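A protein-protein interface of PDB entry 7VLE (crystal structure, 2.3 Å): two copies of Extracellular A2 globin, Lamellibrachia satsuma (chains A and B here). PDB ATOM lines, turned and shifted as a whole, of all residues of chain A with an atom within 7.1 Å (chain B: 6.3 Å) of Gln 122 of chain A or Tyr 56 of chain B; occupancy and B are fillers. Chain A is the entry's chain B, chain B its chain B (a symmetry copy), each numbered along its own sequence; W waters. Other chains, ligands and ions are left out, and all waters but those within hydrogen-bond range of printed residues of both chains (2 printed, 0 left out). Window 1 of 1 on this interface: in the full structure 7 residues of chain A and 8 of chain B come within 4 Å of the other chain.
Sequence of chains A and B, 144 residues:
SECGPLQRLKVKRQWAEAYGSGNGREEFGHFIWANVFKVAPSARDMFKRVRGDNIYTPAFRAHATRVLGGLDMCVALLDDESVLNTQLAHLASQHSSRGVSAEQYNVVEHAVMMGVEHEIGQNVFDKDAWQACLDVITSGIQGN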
ATOM      1  N   MET A 113     -13.047   6.228  -0.470  1.00  0.00           N
ATOM      2  CA  MET A 113     -13.123   6.418   0.975  1.00  0.00           C
ATOM      3  C   MET A 113     -11.750   6.308   1.626  1.00  0.00           C
ATOM      4  O   MET A 113     -11.423   7.086   2.528  1.00  0.00           O
ATOM      5  CB  MET A 113     -14.093   5.405   1.585  1.00  0.00           C
ATOM      6  CG  MET A 113     -15.544   5.652   1.213  1.00  0.00           C
ATOM      7  SD  MET A 113     -16.723   4.603   2.084  1.00  0.00           S
ATOM      8  CE  MET A 113     -16.293   2.987   1.444  1.00  0.00           C
ATOM      9  N   MET A 114     -10.938   5.341   1.193  1.00  0.00           N
ATOM     10  CA  MET A 114      -9.570   5.262   1.693  1.00  0.00           C
ATOM     11  C   MET A 114      -8.758   6.477   1.268  1.00  0.00           C
ATOM     12  O   MET A 114      -7.861   6.911   1.998  1.00  0.00           O
ATOM     13  CB  MET A 114      -8.897   3.977   1.205  1.00  0.00           C
ATOM     14  CG  MET A 114      -9.482   2.686   1.774  1.00  0.00           C
ATOM     15  SD  MET A 114      -9.168   2.444   3.536  1.00  0.00           S
ATOM     16  CE  MET A 114     -10.692   3.057   4.253  1.00  0.00           C
ATOM     17  N   VAL A 116      -9.923   9.679   0.724  1.00  0.00           N
ATOM     18  CA  VAL A 116     -10.308  10.839   1.528  1.00  0.00           C
ATOM     19  C   VAL A 116      -9.739  10.721   2.932  1.00  0.00           C
ATOM     20  O   VAL A 116      -9.228  11.695   3.499  1.00  0.00           O
ATOM     21  CB  VAL A 116     -11.840  10.988   1.558  1.00  0.00           C
ATOM     22  CG1 VAL A 116     -12.249  12.088   2.528  1.00  0.00           C
ATOM     23  CG2 VAL A 116     -12.382  11.269   0.169  1.00  0.00           C
ATOM     24  N   GLU A 117      -9.833   9.527   3.522  1.00  0.00           N
ATOM     25  CA  GLU A 117      -9.259   9.289   4.841  1.00  0.00           C
ATOM     26  C   GLU A 117      -7.751   9.499   4.825  1.00  0.00           C
ATOM     27  O   GLU A 117      -7.190  10.115   5.739  1.00  0.00           O
ATOM     28  CB  GLU A 117      -9.603   7.873   5.301  1.00  0.00           C
ATOM     29  CG  GLU A 117      -9.287   7.601   6.757  1.00  0.00           C
ATOM     30  CD  GLU A 117      -8.326   6.445   6.942  1.00  0.00           C
ATOM     31  OE1 GLU A 117      -8.776   5.349   7.337  1.00  0.00           O
ATOM     32  OE2 GLU A 117      -7.119   6.633   6.687  1.00  0.00           O
ATOM     33  N   HIS A 118      -7.080   8.991   3.787  1.00  0.00           N
ATOM     34  CA  HIS A 118      -5.642   9.195   3.640  1.00  0.00           C
ATOM     35  C   HIS A 118      -5.301  10.668   3.463  1.00  0.00           C
ATOM     36  O   HIS A 118      -4.196  11.099   3.816  1.00  0.00           O
ATOM     37  CB  HIS A 118      -5.136   8.371   2.454  1.00  0.00           C
ATOM     38  CG  HIS A 118      -3.962   8.969   1.744  1.00  0.00           C
ATOM     39  ND1 HIS A 118      -2.670   8.849   2.208  1.00  0.00           N
ATOM     40  CD2 HIS A 118      -3.884   9.682   0.595  1.00  0.00           C
ATOM     41  CE1 HIS A 118      -1.847   9.466   1.380  1.00  0.00           C
ATOM     42  NE2 HIS A 118      -2.559   9.980   0.392  1.00  0.00           N
ATOM     43  N   GLU A 119      -6.239  11.456   2.941  1.00  0.00           N
ATOM     44  CA  GLU A 119      -6.007  12.866   2.664  1.00  0.00           C
ATOM     45  C   GLU A 119      -6.304  13.754   3.867  1.00  0.00           C
ATOM     46  O   GLU A 119      -5.613  14.755   4.081  1.00  0.00           O
ATOM     47  CB  GLU A 119      -6.854  13.303   1.468  1.00  0.00           C
ATOM     48  CG  GLU A 119      -6.145  14.251   0.523  1.00  0.00           C
ATOM     49  CD  GLU A 119      -4.861  13.664  -0.035  1.00  0.00           C
ATOM     50  OE1 GLU A 119      -4.931  12.670  -0.790  1.00  0.00           O
ATOM     51  OE2 GLU A 119      -3.780  14.195   0.291  1.00  0.00           O
ATOM     52  N   ILE A 120      -7.318  13.411   4.661  1.00  0.00           N
ATOM     53  CA  ILE A 120      -7.710  14.227   5.807  1.00  0.00           C
ATOM     54  C   ILE A 120      -7.355  13.588   7.139  1.00  0.00           C
ATOM     55  O   ILE A 120      -7.404  14.280   8.170  1.00  0.00           O
ATOM     56  CB  ILE A 120      -9.215  14.565   5.773  1.00  0.00           C
ATOM     57  CG1 ILE A 120     -10.049  13.327   6.111  1.00  0.00           C
ATOM     58  CG2 ILE A 120      -9.604  15.115   4.411  1.00  0.00           C
ATOM     59  CD1 ILE A 120     -11.542  13.568   6.070  1.00  0.00           C
ATOM     60  N   GLY A 121      -7.005  12.303   7.161  1.00  0.00           N
ATOM     61  CA  GLY A 121      -6.639  11.640   8.396  1.00  0.00           C
ATOM     62  C   GLY A 121      -7.733  10.748   8.944  1.00  0.00           C
ATOM     63  O   GLY A 121      -8.912  11.115   8.920  1.00  0.00           O
ATOM     64  N   GLN A 122      -7.352   9.567   9.439  1.00  0.00           N
ATOM     65  CA  GLN A 122      -8.306   8.679  10.096  1.00  0.00           C
ATOM     66  C   GLN A 122      -8.923   9.323  11.327  1.00  0.00           C
ATOM     67  O   GLN A 122     -10.004   8.909  11.763  1.00  0.00           O
ATOM     68  CB  GLN A 122      -7.615   7.367  10.483  1.00  0.00           C
ATOM     69  CG  GLN A 122      -6.407   7.533  11.410  1.00  0.00           C
ATOM     70  CD  GLN A 122      -6.793   7.651  12.876  1.00  0.00           C
ATOM     71  OE1 GLN A 122      -7.824   7.128  13.301  1.00  0.00           O
ATOM     72  NE2 GLN A 122      -5.971   8.348  13.652  1.00  0.00           N
ATOM     73  N   ASN A 123      -8.254  10.332  11.881  1.00  0.00           N
ATOM     74  CA  ASN A 123      -8.671  10.956  13.131  1.00  0.00           C
ATOM     75  C   ASN A 123      -9.999  11.694  12.993  1.00  0.00           C
ATOM     76  O   ASN A 123     -10.721  11.854  13.984  1.00  0.00           O
ATOM     77  CB  ASN A 123      -7.560  11.900  13.595  1.00  0.00           C
ATOM     78  CG  ASN A 123      -7.967  12.756  14.766  1.00  0.00           C
ATOM     79  OD1 ASN A 123      -8.148  12.261  15.878  1.00  0.00           O
ATOM     80  ND2 ASN A 123      -8.093  14.056  14.531  1.00  0.00           N
ATOM     81  N   VAL A 124     -10.344  12.139  11.788  1.00  0.00           N
ATOM     82  CA  VAL A 124     -11.569  12.897  11.561  1.00  0.00           C
ATOM     83  C   VAL A 124     -12.522  12.211  10.595  1.00  0.00           C
ATOM     84  O   VAL A 124     -13.691  12.617  10.513  1.00  0.00           O
ATOM     85  CB  VAL A 124     -11.262  14.325  11.060  1.00  0.00           C
ATOM     86  CG1 VAL A 124     -10.404  15.074  12.068  1.00  0.00           C
ATOM     87  CG2 VAL A 124     -10.580  14.271   9.702  1.00  0.00           C
ATOM     88  N   PHE A 125     -12.070  11.187   9.874  1.00  0.00           N
ATOM     89  CA  PHE A 125     -12.858  10.595   8.800  1.00  0.00           C
ATOM     90  C   PHE A 125     -14.157   9.989   9.323  1.00  0.00           C
ATOM     91  O   PHE A 125     -14.149   9.165  10.243  1.00  0.00           O
ATOM     92  CB  PHE A 125     -12.028   9.530   8.087  1.00  0.00           C
ATOM     93  CG  PHE A 125     -12.729   8.894   6.928  1.00  0.00           C
ATOM     94  CD1 PHE A 125     -12.914   9.594   5.750  1.00  0.00           C
ATOM     95  CD2 PHE A 125     -13.198   7.595   7.014  1.00  0.00           C
ATOM     96  CE1 PHE A 125     -13.560   9.013   4.677  1.00  0.00           C
ATOM     97  CE2 PHE A 125     -13.844   7.007   5.944  1.00  0.00           C
ATOM     98  CZ  PHE A 125     -14.026   7.718   4.774  1.00  0.00           C
ATOM     99  N   ASP A 126     -15.274  10.394   8.717  1.00  0.00           N
ATOM    100  CA  ASP A 126     -16.613   9.945   9.101  1.00  0.00           C
ATOM    101  C   ASP A 126     -17.034   8.833   8.142  1.00  0.00           C
ATOM    102  O   ASP A 126     -17.616   9.085   7.086  1.00  0.00           O
ATOM    103  CB  ASP A 126     -17.597  11.112   9.075  1.00  0.00           C
ATOM    104  CG  ASP A 126     -18.924  10.784   9.743  1.00  0.00           C
ATOM    105  OD1 ASP A 126     -19.546  11.706  10.309  1.00  0.00           O
ATOM    106  OD2 ASP A 126     -19.346   9.609   9.713  1.00  0.00           O
ATOM    107  N   LYS A 127     -16.762   7.585   8.537  1.00  0.00           N
ATOM    108  CA  LYS A 127     -17.008   6.443   7.657  1.00  0.00           C
ATOM    109  C   LYS A 127     -18.493   6.245   7.377  1.00  0.00           C
ATOM    110  O   LYS A 127     -18.879   5.942   6.242  1.00  0.00           O
ATOM    111  CB  LYS A 127     -16.412   5.174   8.269  1.00  0.00           C
ATOM    112  CG  LYS A 127     -16.689   3.909   7.468  1.00  0.00           C
ATOM    113  CD  LYS A 127     -16.106   2.678   8.146  1.00  0.00           C
ATOM    114  CE  LYS A 127     -16.408   1.411   7.356  1.00  0.00           C
ATOM    115  NZ  LYS A 127     -17.870   1.153   7.247  1.00  0.00           N
ATOM    116  N   ASP A 128     -19.341   6.393   8.399  1.00  0.00           N
ATOM    117  CA  ASP A 128     -20.774   6.177   8.216  1.00  0.00           C
ATOM    118  C   ASP A 128     -21.368   7.200   7.255  1.00  0.00           C
ATOM    119  O   ASP A 128     -22.140   6.850   6.356  1.00  0.00           O
ATOM    120  CB  ASP A 128     -21.495   6.235   9.564  1.00  0.00           C
ATOM    121  CG  ASP A 128     -21.344   4.958  10.364  1.00  0.00           C
ATOM    122  OD1 ASP A 128     -21.175   3.883   9.750  1.00  0.00           O
ATOM    123  OD2 ASP A 128     -21.401   5.028  11.610  1.00  0.00           O
ATOM    124  N   GLU B  26      -4.319   6.640  19.775  1.00  0.00           N
ATOM    125  CA  GLU B  26      -5.475   6.469  18.899  1.00  0.00           C
ATOM    126  C   GLU B  26      -5.047   6.034  17.504  1.00  0.00           C
ATOM    127  O   GLU B  26      -5.673   5.156  16.899  1.00  0.00           O
ATOM    128  CB  GLU B  26      -6.283   7.762  18.820  1.00  0.00           C
ATOM    129  CG  GLU B  26      -7.542   7.628  17.977  1.00  0.00           C
ATOM    130  CD  GLU B  26      -8.154   8.964  17.607  1.00  0.00           C
ATOM    131  OE1 GLU B  26      -7.682   9.588  16.636  1.00  0.00           O
ATOM    132  OE2 GLU B  26      -9.109   9.388  18.291  1.00  0.00           O
ATOM    133  N   GLU B  27      -3.989   6.651  16.974  1.00  0.00           N
ATOM    134  CA  GLU B  27      -3.464   6.249  15.674  1.00  0.00           C
ATOM    135  C   GLU B  27      -2.813   4.875  15.752  1.00  0.00           C
ATOM    136  O   GLU B  27      -2.925   4.072  14.819  1.00  0.00           O
ATOM    137  CB  GLU B  27      -2.463   7.295  15.177  1.00  0.00           C
ATOM    138  CG  GLU B  27      -1.988   7.114  13.740  1.00  0.00           C
ATOM    139  CD  GLU B  27      -0.870   6.093  13.598  1.00  0.00           C
ATOM    140  OE1 GLU B  27      -0.672   5.585  12.474  1.00  0.00           O
ATOM    141  OE2 GLU B  27      -0.193   5.797  14.606  1.00  0.00           O
ATOM    142  N   PHE B  28      -2.114   4.602  16.856  1.00  0.00           N
ATOM    143  CA  PHE B  28      -1.488   3.300  17.062  1.00  0.00           C
ATOM    144  C   PHE B  28      -2.521   2.184  17.000  1.00  0.00           C
ATOM    145  O   PHE B  28      -2.356   1.206  16.260  1.00  0.00           O
ATOM    146  CB  PHE B  28      -0.767   3.293  18.411  1.00  0.00           C
ATOM    147  CG  PHE B  28       0.059   2.065  18.659  1.00  0.00           C
ATOM    148  CD1 PHE B  28       0.285   1.622  19.951  1.00  0.00           C
ATOM    149  CD2 PHE B  28       0.630   1.368  17.607  1.00  0.00           C
ATOM    150  CE1 PHE B  28       1.050   0.497  20.192  1.00  0.00           C
ATOM    151  CE2 PHE B  28       1.397   0.241  17.841  1.00  0.00           C
ATOM    152  CZ  PHE B  28       1.607  -0.193  19.135  1.00  0.00           C
ATOM    153  N   HIS B  30      -5.573   2.319  15.770  1.00  0.00           N
ATOM    154  CA  HIS B  30      -6.244   2.286  14.475  1.00  0.00           C
ATOM    155  C   HIS B  30      -5.433   1.498  13.456  1.00  0.00           C
ATOM    156  O   HIS B  30      -5.975   0.658  12.729  1.00  0.00           O
ATOM    157  CB  HIS B  30      -6.485   3.701  13.952  1.00  0.00           C
ATOM    158  CG  HIS B  30      -7.007   3.729  12.549  1.00  0.00           C
ATOM    159  ND1 HIS B  30      -8.345   3.581  12.251  1.00  0.00           N
ATOM    160  CD2 HIS B  30      -6.369   3.849  11.361  1.00  0.00           C
ATOM    161  CE1 HIS B  30      -8.510   3.628  10.942  1.00  0.00           C
ATOM    162  NE2 HIS B  30      -7.326   3.789  10.378  1.00  0.00           N
ATOM    163  N   ARG B  51     -19.060  -2.069  17.530  1.00  0.00           N
ATOM    164  CA  ARG B  51     -19.061  -1.459  16.198  1.00  0.00           C
ATOM    165  C   ARG B  51     -17.830  -1.875  15.386  1.00  0.00           C
ATOM    166  O   ARG B  51     -17.073  -1.040  14.885  1.00  0.00           O
ATOM    167  CB  ARG B  51     -19.151   0.070  16.291  1.00  0.00           C
ATOM    168  CG  ARG B  51     -20.402   0.609  16.962  1.00  0.00           C
ATOM    169  CD  ARG B  51     -21.642   0.342  16.127  1.00  0.00           C
ATOM    170  NE  ARG B  51     -21.414   0.587  14.707  1.00  0.00           N
ATOM    171  CZ  ARG B  51     -21.482   1.781  14.128  1.00  0.00           C
ATOM    172  NH1 ARG B  51     -21.769   2.857  14.848  1.00  0.00           N
ATOM    173  NH2 ARG B  51     -21.261   1.901  12.826  1.00  0.00           N
ATOM    174  N   ASN B  54     -17.276  -0.330  11.952  1.00  0.00           N
ATOM    175  CA  ASN B  54     -16.786   1.044  11.799  1.00  0.00           C
ATOM    176  C   ASN B  54     -15.776   1.331  12.908  1.00  0.00           C
ATOM    177  O   ASN B  54     -16.141   1.805  13.986  1.00  0.00           O
ATOM    178  CB  ASN B  54     -17.948   2.029  11.828  1.00  0.00           C
ATOM    179  CG  ASN B  54     -17.522   3.444  11.504  1.00  0.00           C
ATOM    180  OD1 ASN B  54     -16.335   3.754  11.458  1.00  0.00           O
ATOM    181  ND2 ASN B  54     -18.498   4.314  11.286  1.00  0.00           N
ATOM    182  N   ILE B  55     -14.499   1.088  12.622  1.00  0.00           N
ATOM    183  CA  ILE B  55     -13.441   1.256  13.615  1.00  0.00           C
ATOM    184  C   ILE B  55     -13.115   2.730  13.844  1.00  0.00           C
ATOM    185  O   ILE B  55     -12.212   3.063  14.622  1.00  0.00           O
ATOM    186  CB  ILE B  55     -12.166   0.494  13.217  1.00  0.00           C
ATOM    187  CG1 ILE B  55     -11.466   1.183  12.045  1.00  0.00           C
ATOM    188  CG2 ILE B  55     -12.493  -0.950  12.884  1.00  0.00           C
ATOM    189  CD1 ILE B  55     -10.107   0.596  11.727  1.00  0.00           C
ATOM    190  N   TYR B  56     -13.831   3.627  13.164  1.00  0.00           N
ATOM    191  CA  TYR B  56     -13.677   5.057  13.405  1.00  0.00           C
ATOM    192  C   TYR B  56     -14.575   5.558  14.529  1.00  0.00           C
ATOM    193  O   TYR B  56     -14.369   6.673  15.022  1.00  0.00           O
ATOM    194  CB  TYR B  56     -13.961   5.844  12.118  1.00  0.00           C
ATOM    195  CG  TYR B  56     -13.096   5.431  10.943  1.00  0.00           C
ATOM    196  CD1 TYR B  56     -11.882   6.060  10.695  1.00  0.00           C
ATOM    197  CD2 TYR B  56     -13.494   4.417  10.082  1.00  0.00           C
ATOM    198  CE1 TYR B  56     -11.088   5.688   9.622  1.00  0.00           C
ATOM    199  CE2 TYR B  56     -12.708   4.038   9.008  1.00  0.00           C
ATOM    200  CZ  TYR B  56     -11.507   4.676   8.782  1.00  0.00           C
ATOM    201  OH  TYR B  56     -10.725   4.300   7.715  1.00  0.00           O
ATOM    202  N   THR B  57     -15.545   4.749  14.952  1.00  0.00           N
ATOM    203  CA  THR B  57     -16.486   5.155  15.981  1.00  0.00           C
ATOM    204  C   THR B  57     -15.805   5.242  17.346  1.00  0.00           C
ATOM    205  O   THR B  57     -14.851   4.510  17.624  1.00  0.00           O
ATOM    206  CB  THR B  57     -17.650   4.169  16.069  1.00  0.00           C
ATOM    207  OG1 THR B  57     -17.151   2.863  16.386  1.00  0.00           O
ATOM    208  CG2 THR B  57     -18.411   4.116  14.755  1.00  0.00           C
ATOM    209  N   PRO B  58     -16.288   6.132  18.218  1.00  0.00           N
ATOM    210  CA  PRO B  58     -15.789   6.153  19.603  1.00  0.00           C
ATOM    211  C   PRO B  58     -15.978   4.830  20.315  1.00  0.00           C
ATOM    212  O   PRO B  58     -15.200   4.497  21.220  1.00  0.00           O
ATOM    213  CB  PRO B  58     -16.624   7.264  20.258  1.00  0.00           C
ATOM    214  CG  PRO B  58     -17.138   8.092  19.118  1.00  0.00           C
ATOM    215  CD  PRO B  58     -17.320   7.153  17.975  1.00  0.00           C
ATOM    216  N   ALA B  59     -16.999   4.064  19.923  1.00  0.00           N
ATOM    217  CA  ALA B  59     -17.264   2.774  20.547  1.00  0.00           C
ATOM    218  C   ALA B  59     -16.116   1.800  20.308  1.00  0.00           C
ATOM    219  O   ALA B  59     -15.662   1.120  21.234  1.00  0.00           O
ATOM    220  CB  ALA B  59     -18.575   2.201  20.012  1.00  0.00           C
ATOM    221  N   PHE B  60     -15.638   1.715  19.065  1.00  0.00           N
ATOM    222  CA  PHE B  60     -14.542   0.801  18.769  1.00  0.00           C
ATOM    223  C   PHE B  60     -13.202   1.342  19.245  1.00  0.00           C
ATOM    224  O   PHE B  60     -12.333   0.559  19.646  1.00  0.00           O
ATOM    225  CB  PHE B  60     -14.468   0.507  17.272  1.00  0.00           C
ATOM    226  CG  PHE B  60     -13.489  -0.580  16.927  1.00  0.00           C
ATOM    227  CD1 PHE B  60     -13.880  -1.908  16.951  1.00  0.00           C
ATOM    228  CD2 PHE B  60     -12.177  -0.278  16.599  1.00  0.00           C
ATOM    229  CE1 PHE B  60     -12.985  -2.914  16.644  1.00  0.00           C
ATOM    230  CE2 PHE B  60     -11.276  -1.280  16.290  1.00  0.00           C
ATOM    231  CZ  PHE B  60     -11.681  -2.600  16.312  1.00  0.00           C
ATOM    232  N   ARG B  61     -13.011   2.662  19.188  1.00  0.00           N
ATOM    233  CA  ARG B  61     -11.766   3.244  19.672  1.00  0.00           C
ATOM    234  C   ARG B  61     -11.566   2.962  21.154  1.00  0.00           C
ATOM    235  O   ARG B  61     -10.425   2.814  21.610  1.00  0.00           O
ATOM    236  CB  ARG B  61     -11.748   4.751  19.403  1.00  0.00           C
ATOM    237  CG  ARG B  61     -11.769   5.121  17.926  1.00  0.00           C
ATOM    238  CD  ARG B  61     -11.547   6.614  17.725  1.00  0.00           C
ATOM    239  NE  ARG B  61     -11.729   7.023  16.334  1.00  0.00           N
ATOM    240  CZ  ARG B  61     -10.785   6.951  15.400  1.00  0.00           C
ATOM    241  NH1 ARG B  61     -11.044   7.351  14.161  1.00  0.00           N
ATOM    242  NH2 ARG B  61      -9.584   6.477  15.700  1.00  0.00           N
HETATM  243  O   HOH W   1     -12.765   9.302  12.279  1.00  0.00           O
HETATM  244  O   HOH W   2      -7.250   3.209   7.925  1.00  0.00           O
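The backbone carbonyl oxygen (O) of Gln 122 of chain A lies within hydrogen-bond range of the guanidinium group (NH1) of Arg 61 of chain B. The side-chain amide oxygen (OD1) of Asn 123 of chain A sits close to the side-chain carboxylate (OE1) of Glu 26 of chain B, at 2.8 Å. NH2 of Arg 51 of chain B is in salt-bridge range of OD2 of Asp 128 of chain A, 3.4 Å away. The side-chain carboxylate (OD2) of Asp 128 of chain A lies within hydrogen-bond range of the side-chain amide nitrogen (ND2) of Asn 54 of chain B (3.0 Å). The side-chain carboxylate (OE1) of Glu 117 of chain A sits close to the side-chain hydroxyl (OH) of Tyr 56 of chain B (2.2 Å).
The backbone NH of Asp 128 of chain A sits close to the side-chain carboxylate of Asp 126 of chain A. The side-chain carboxylate (OE1) of Glu 26 of chain B lies within salt-bridge range of the guanidinium group (NH2) of Arg 61 of chain B. OD1 of Asn 54 of chain B sits close to N of Tyr 56 of chain B, at 3.0 Å. O of Asn 54 of chain B is in hydrogen-bond range of OG1 of Thr 57 of chain B (2.8 Å). The backbone carbonyl oxygen (O) of Tyr 56 of chain B is in hydrogen-bond range of the guanidinium group (NE) of Arg 61 of chain B (3.0 Å).
Among the printed residues, pairs that only touch across the chains: Lys 127 of chain A with Asn 54 of chain B, Lys 127 of chain A with Tyr 56 of chain B, Gln 122 of chain A with Tyr 56 of chain B, Gln 122 of chain A with His 30 of chain B, Gln 122 of chain A with Glu 26 of chain B, Met 114 of chain A with Tyr 56 of chain B, Glu 117 of chain A with His 30 of chain B, Phe 125 of chain A with Tyr 56 of chain B and Gln 122 of chain A with Glu 27 of chain B.
Gln 122 of chain A touches just these residues of chain B: Glu 26 (3.7 Å), Glu 27 (3.8 Å), His 30 (3.6 Å), Tyr 56 (3.6 Å) and Arg 61 (3.0 Å). Of the printed residues of chain A, Glu 26 of chain B touches Gln 122 (3.7 Å) and Asn 123 (2.8 Å). Printed residues of chain A within 4 Å of Glu 27 of chain B: Gln 122. Printed residues of chain A within 4 Å of Tyr 56 of chain B: Met 114, Glu 117, Gln 122, Phe 125 and Lys 127. Thr 57 of chain B touches none of the printed residues of chain A. The nearest printed residue of chain A that does not touch Tyr 56 of chain B is Asn 123 of chain A (5.7 Å). The nearest printed residue of chain B that does not touch Glu 117 of chain A is Ile 55 of chain B (6.6 Å).
Of the 13 printed residues of chain B, 7 touch a printed residue of chain A. Hydrophobic or aromatic side chains of chain B within 4 Å of the printed part of chain A: His 30 and Tyr 56.
No position is printed for both chains.
Water W1 lies within hydrogen-bond range of the backbone carbonyl oxygen of Phe 125 of chain A (2.5 Å), the backbone carbonyl oxygen of Gln 122 of chain A (2.8 Å) and the guanidinium group of Arg 61 of chain B (3.2 Å). Water W2 bridges a ring nitrogen (NE2) of His 30 of chain B and the side-chain carboxylate (OE1) of Glu 117 of chain A.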
